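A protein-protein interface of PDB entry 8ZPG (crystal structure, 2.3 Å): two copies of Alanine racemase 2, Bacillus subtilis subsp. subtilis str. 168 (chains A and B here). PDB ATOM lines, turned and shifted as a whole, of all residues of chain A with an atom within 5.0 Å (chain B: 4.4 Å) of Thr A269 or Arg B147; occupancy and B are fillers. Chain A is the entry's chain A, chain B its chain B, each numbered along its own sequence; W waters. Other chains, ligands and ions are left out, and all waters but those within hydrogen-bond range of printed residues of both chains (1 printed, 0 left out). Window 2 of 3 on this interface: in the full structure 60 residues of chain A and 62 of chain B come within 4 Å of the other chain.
Water W1 lies within hydrogen-bond range of NH1 of Arg B147 (2.9 Å) and O of Pro A271 (3.0 Å).
The backbone carbonyl oxygen of Met A267 is in hydrogen-bond range of the guanidinium group of Arg A272 (3.2 Å). The guanidinium group (NH1) of Arg A272 lies within salt-bridge range of the side-chain carboxylate (OE1) of Glu A270, 3.9 Å away. The side-chain carboxylate of Asp B138 is in hydrogen-bond range of the backbone NH of Gly B142, at 2.9 Å. The side-chain carboxylate (OD2) of Asp B138 lies within salt-bridge range of the guanidinium group (NH1) of Arg B147 (3.0 Å). N of Arg B147 is in hydrogen-bond range of OE2 of Glu B151, 3.0 Å away. The side-chain hydroxyl (OG1) of Thr B148 sits at hydrogen-bond distance from the backbone NH (N) of Glu B151, 3.2 Å away.
Of the 9 printed residues of chain B, 4 touch a printed residue of chain A.
CE of Met A267 touches NH1 of Arg B147 (3.4 Å). O of Thr A269 touches NH2 of Arg B147, 3.6 Å away. Thr A269 touches Thr B148. Thr A269 touches Lys B191.
NZ of Lys A265 lies within hydrogen-bond range of O of Gly B142 (2.8 Å). The backbone carbonyl oxygen (O) of Glu A270 sits at hydrogen-bond distance from the side-chain amino group (NZ) of Lys B191. O of Pro A271 lies within hydrogen-bond range of NH2 of Arg B147, 2.6 Å away.
Of the printed residues of chain B, Lys A265 touches Gly B142. Of the printed residues of chain B, Met A267 touches Arg B147. Of chain B, only Arg B147, Thr B148 and Lys B191 come within 4 Å of Thr A269. Printed residues of chain B within 4 Å of Glu A270: Lys B191 (3.3 Å). Of the printed residues of chain A, Gly B142 touches Lys A265 (2.8 Å). Of chain A, only Met A267 (3.4 Å), Thr A269 (3.6 Å) and Pro A271 (2.6 Å) come within 4 Å of Arg B147. Of the printed residues of chain A, Thr B148 touches Thr A269 (3.6 Å). The nearest printed residue of chain B that does not touch Thr A269 is Asp B138 (6.4 Å).
No position is printed for both chains. Of the 7 pairs that touch across the chains among the printed residues, none has its exchanged pair printed and touching as well.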
ATOM      1  N   LYS A 265      39.873 -25.070   7.816  1.00  0.00           N
ATOM      2  CA  LYS A 265      38.568 -25.325   7.196  1.00  0.00           C
ATOM      3  C   LYS A 265      38.577 -25.018   5.696  1.00  0.00           C
ATOM      4  O   LYS A 265      39.319 -24.153   5.227  1.00  0.00           O
ATOM      5  CB  LYS A 265      37.457 -24.504   7.869  1.00  0.00           C
ATOM      6  CG  LYS A 265      37.499 -23.001   7.571  1.00  0.00           C
ATOM      7  CD  LYS A 265      36.419 -22.231   8.319  1.00  0.00           C
ATOM      8  CE  LYS A 265      36.600 -20.708   8.209  1.00  0.00           C
ATOM      9  NZ  LYS A 265      37.227 -20.108   9.422  1.00  0.00           N
ATOM     10  N   MET A 267      36.215 -23.651   2.529  1.00  0.00           N
ATOM     11  CA  MET A 267      35.109 -22.699   2.370  1.00  0.00           C
ATOM     12  C   MET A 267      34.101 -23.211   1.334  1.00  0.00           C
ATOM     13  O   MET A 267      33.996 -22.710   0.213  1.00  0.00           O
ATOM     14  CB  MET A 267      35.651 -21.330   1.973  1.00  0.00           C
ATOM     15  CG  MET A 267      36.761 -20.784   2.884  1.00  0.00           C
ATOM     16  SD  MET A 267      36.213 -20.464   4.577  1.00  0.00           S
ATOM     17  CE  MET A 267      34.892 -19.283   4.348  1.00  0.00           C
ATOM     18  N   ARG A 268      33.320 -24.214   1.747  1.00  0.00           N
ATOM     19  CA  ARG A 268      32.420 -24.941   0.831  1.00  0.00           C
ATOM     20  C   ARG A 268      31.020 -24.337   0.787  1.00  0.00           C
ATOM     21  O   ARG A 268      30.578 -23.841  -0.253  1.00  0.00           O
ATOM     22  CB  ARG A 268      32.355 -26.413   1.230  1.00  0.00           C
ATOM     23  CG  ARG A 268      32.012 -27.299   0.080  1.00  0.00           C
ATOM     24  CD  ARG A 268      33.028 -27.139  -1.044  1.00  0.00           C
ATOM     25  NE  ARG A 268      32.608 -27.843  -2.251  1.00  0.00           N
ATOM     26  CZ  ARG A 268      32.188 -29.103  -2.281  1.00  0.00           C
ATOM     27  NH1 ARG A 268      32.164 -29.856  -1.190  1.00  0.00           N
ATOM     28  NH2 ARG A 268      31.784 -29.624  -3.437  1.00  0.00           N
ATOM     29  N   THR A 269      30.298 -24.406   1.899  1.00  0.00           N
ATOM     30  CA  THR A 269      29.042 -23.682   2.021  1.00  0.00           C
ATOM     31  C   THR A 269      29.292 -22.196   1.733  1.00  0.00           C
ATOM     32  O   THR A 269      30.429 -21.757   1.574  1.00  0.00           O
ATOM     33  CB  THR A 269      28.450 -23.913   3.418  1.00  0.00           C
ATOM     34  OG1 THR A 269      28.599 -22.737   4.228  1.00  0.00           O
ATOM     35  CG2 THR A 269      29.192 -25.058   4.117  1.00  0.00           C
ATOM     36  N   GLU A 270      28.226 -21.412   1.652  1.00  0.00           N
ATOM     37  CA  GLU A 270      28.378 -19.967   1.572  1.00  0.00           C
ATOM     38  C   GLU A 270      27.436 -19.270   2.543  1.00  0.00           C
ATOM     39  O   GLU A 270      26.505 -19.888   3.071  1.00  0.00           O
ATOM     40  CB  GLU A 270      28.152 -19.442   0.146  1.00  0.00           C
ATOM     41  CG  GLU A 270      26.750 -19.501  -0.386  1.00  0.00           C
ATOM     42  CD  GLU A 270      26.698 -19.042  -1.833  1.00  0.00           C
ATOM     43  OE1 GLU A 270      27.200 -17.930  -2.128  1.00  0.00           O
ATOM     44  OE2 GLU A 270      26.173 -19.800  -2.677  1.00  0.00           O
ATOM     45  N   PRO A 271      27.667 -17.967   2.818  1.00  0.00           N
ATOM     46  CA  PRO A 271      28.688 -17.106   2.195  1.00  0.00           C
ATOM     47  C   PRO A 271      30.145 -17.434   2.559  1.00  0.00           C
ATOM     48  O   PRO A 271      30.425 -18.040   3.601  1.00  0.00           O
ATOM     49  CB  PRO A 271      28.317 -15.706   2.699  1.00  0.00           C
ATOM     50  CG  PRO A 271      27.641 -15.936   3.983  1.00  0.00           C
ATOM     51  CD  PRO A 271      26.908 -17.250   3.859  1.00  0.00           C
ATOM     52  N   ARG A 272      31.065 -17.025   1.680  1.00  0.00           N
ATOM     53  CA  ARG A 272      32.494 -17.295   1.815  1.00  0.00           C
ATOM     54  C   ARG A 272      33.296 -16.025   2.113  1.00  0.00           C
ATOM     55  O   ARG A 272      34.404 -15.834   1.610  1.00  0.00           O
ATOM     56  CB  ARG A 272      33.029 -17.974   0.559  1.00  0.00           C
ATOM     57  CG  ARG A 272      32.075 -18.983  -0.060  1.00  0.00           C
ATOM     58  CD  ARG A 272      32.647 -19.556  -1.365  1.00  0.00           C
ATOM     59  NE  ARG A 272      32.141 -20.896  -1.642  1.00  0.00           N
ATOM     60  CZ  ARG A 272      31.031 -21.151  -2.324  1.00  0.00           C
ATOM     61  NH1 ARG A 272      30.307 -20.177  -2.857  1.00  0.00           N
ATOM     62  NH2 ARG A 272      30.631 -22.412  -2.464  1.00  0.00           N
ATOM     63  N   ASP B 138      29.359 -20.078  12.967  1.00  0.00           N
ATOM     64  CA  ASP B 138      29.930 -19.192  11.949  1.00  0.00           C
ATOM     65  C   ASP B 138      28.914 -18.994  10.826  1.00  0.00           C
ATOM     66  O   ASP B 138      28.690 -19.899  10.019  1.00  0.00           O
ATOM     67  CB  ASP B 138      31.240 -19.781  11.411  1.00  0.00           C
ATOM     68  CG  ASP B 138      31.872 -18.927  10.296  1.00  0.00           C
ATOM     69  OD1 ASP B 138      31.436 -17.766  10.093  1.00  0.00           O
ATOM     70  OD2 ASP B 138      32.807 -19.414   9.617  1.00  0.00           O
ATOM     71  N   GLY B 142      33.598 -16.156   9.080  1.00  0.00           N
ATOM     72  CA  GLY B 142      34.692 -17.015   8.662  1.00  0.00           C
ATOM     73  C   GLY B 142      35.927 -17.048   9.549  1.00  0.00           C
ATOM     74  O   GLY B 142      37.034 -17.304   9.049  1.00  0.00           O
ATOM     75  N   GLY B 145      34.120 -21.458  14.436  1.00  0.00           N
ATOM     76  CA  GLY B 145      32.790 -22.005  14.658  1.00  0.00           C
ATOM     77  C   GLY B 145      32.338 -22.966  13.559  1.00  0.00           C
ATOM     78  O   GLY B 145      32.938 -23.067  12.490  1.00  0.00           O
ATOM     79  N   VAL B 146      31.208 -23.689  13.852  1.00  0.00           N
ATOM     80  CA  VAL B 146      30.598 -24.666  12.934  1.00  0.00           C
ATOM     81  C   VAL B 146      29.811 -23.945  11.832  1.00  0.00           C
ATOM     82  O   VAL B 146      29.226 -22.874  12.051  1.00  0.00           O
ATOM     83  CB  VAL B 146      29.685 -25.661  13.695  1.00  0.00           C
ATOM     84  CG1 VAL B 146      30.322 -26.158  15.015  1.00  0.00           C
ATOM     85  CG2 VAL B 146      28.332 -25.032  13.995  1.00  0.00           C
ATOM     86  N   ARG B 147      29.756 -24.551  10.626  1.00  0.00           N
ATOM     87  CA  ARG B 147      29.236 -23.863   9.441  1.00  0.00           C
ATOM     88  C   ARG B 147      27.949 -24.438   8.833  1.00  0.00           C
ATOM     89  O   ARG B 147      27.258 -23.704   8.113  1.00  0.00           O
ATOM     90  CB  ARG B 147      30.313 -23.811   8.341  1.00  0.00           C
ATOM     91  CG  ARG B 147      31.235 -22.600   8.448  1.00  0.00           C
ATOM     92  CD  ARG B 147      32.262 -22.572   7.318  1.00  0.00           C
ATOM     93  NE  ARG B 147      31.744 -21.944   6.107  1.00  0.00           N
ATOM     94  CZ  ARG B 147      31.852 -20.651   5.824  1.00  0.00           C
ATOM     95  NH1 ARG B 147      32.449 -19.805   6.655  1.00  0.00           N
ATOM     96  NH2 ARG B 147      31.347 -20.193   4.680  1.00  0.00           N
ATOM     97  N   THR B 148      27.594 -25.700   9.096  1.00  0.00           N
ATOM     98  CA  THR B 148      26.438 -26.313   8.445  1.00  0.00           C
ATOM     99  C   THR B 148      25.418 -26.848   9.451  1.00  0.00           C
ATOM    100  O   THR B 148      25.773 -27.339  10.527  1.00  0.00           O
ATOM    101  CB  THR B 148      26.880 -27.434   7.505  1.00  0.00           C
ATOM    102  OG1 THR B 148      26.945 -28.660   8.223  1.00  0.00           O
ATOM    103  CG2 THR B 148      28.261 -27.133   6.938  1.00  0.00           C
ATOM    104  N   GLU B 151      26.098 -30.308  10.830  1.00  0.00           N
ATOM    105  CA  GLU B 151      27.231 -30.547  11.728  1.00  0.00           C
ATOM    106  C   GLU B 151      27.031 -29.903  13.103  1.00  0.00           C
ATOM    107  O   GLU B 151      27.569 -30.405  14.093  1.00  0.00           O
ATOM    108  CB  GLU B 151      28.540 -30.089  11.067  1.00  0.00           C
ATOM    109  CG  GLU B 151      29.158 -28.779  11.561  1.00  0.00           C
ATOM    110  CD  GLU B 151      30.492 -28.444  10.842  1.00  0.00           C
ATOM    111  OE1 GLU B 151      31.439 -29.271  10.924  1.00  0.00           O
ATOM    112  OE2 GLU B 151      30.591 -27.359  10.197  1.00  0.00           O
ATOM    113  N   LYS B 191      20.017 -17.018   8.540  1.00  0.00           N
ATOM    114  CA  LYS B 191      20.635 -18.333   8.644  1.00  0.00           C
ATOM    115  C   LYS B 191      20.692 -18.807  10.094  1.00  0.00           C
ATOM    116  O   LYS B 191      20.434 -19.982  10.376  1.00  0.00           O
ATOM    117  CB  LYS B 191      22.031 -18.304   8.023  1.00  0.00           C
ATOM    118  CG  LYS B 191      22.685 -19.680   7.942  1.00  0.00           C
ATOM    119  CD  LYS B 191      23.559 -19.823   6.701  1.00  0.00           C
ATOM    120  CE  LYS B 191      24.780 -20.660   7.027  1.00  0.00           C
ATOM    121  NZ  LYS B 191      25.320 -21.342   5.817  1.00  0.00           N
ATOM    122  N   PHE B 195      18.900 -22.308  11.922  1.00  0.00           N
ATOM    123  CA  PHE B 195      19.610 -23.409  12.560  1.00  0.00           C
ATOM    124  C   PHE B 195      19.029 -23.738  13.926  1.00  0.00           C
ATOM    125  O   PHE B 195      19.069 -24.899  14.356  1.00  0.00           O
ATOM    126  CB  PHE B 195      21.087 -23.050  12.684  1.00  0.00           C
ATOM    127  CG  PHE B 195      21.832 -23.093  11.396  1.00  0.00           C
ATOM    128  CD1 PHE B 195      21.168 -23.287  10.203  1.00  0.00           C
ATOM    129  CD2 PHE B 195      23.210 -22.942  11.377  1.00  0.00           C
ATOM    130  CE1 PHE B 195      21.875 -23.336   9.005  1.00  0.00           C
ATOM    131  CE2 PHE B 195      23.923 -22.989  10.188  1.00  0.00           C
ATOM    132  CZ  PHE B 195      23.259 -23.187   9.002  1.00  0.00           C
HETATM  133  O   HOH W   1      32.299 -17.056   5.746  1.00  0.00           O
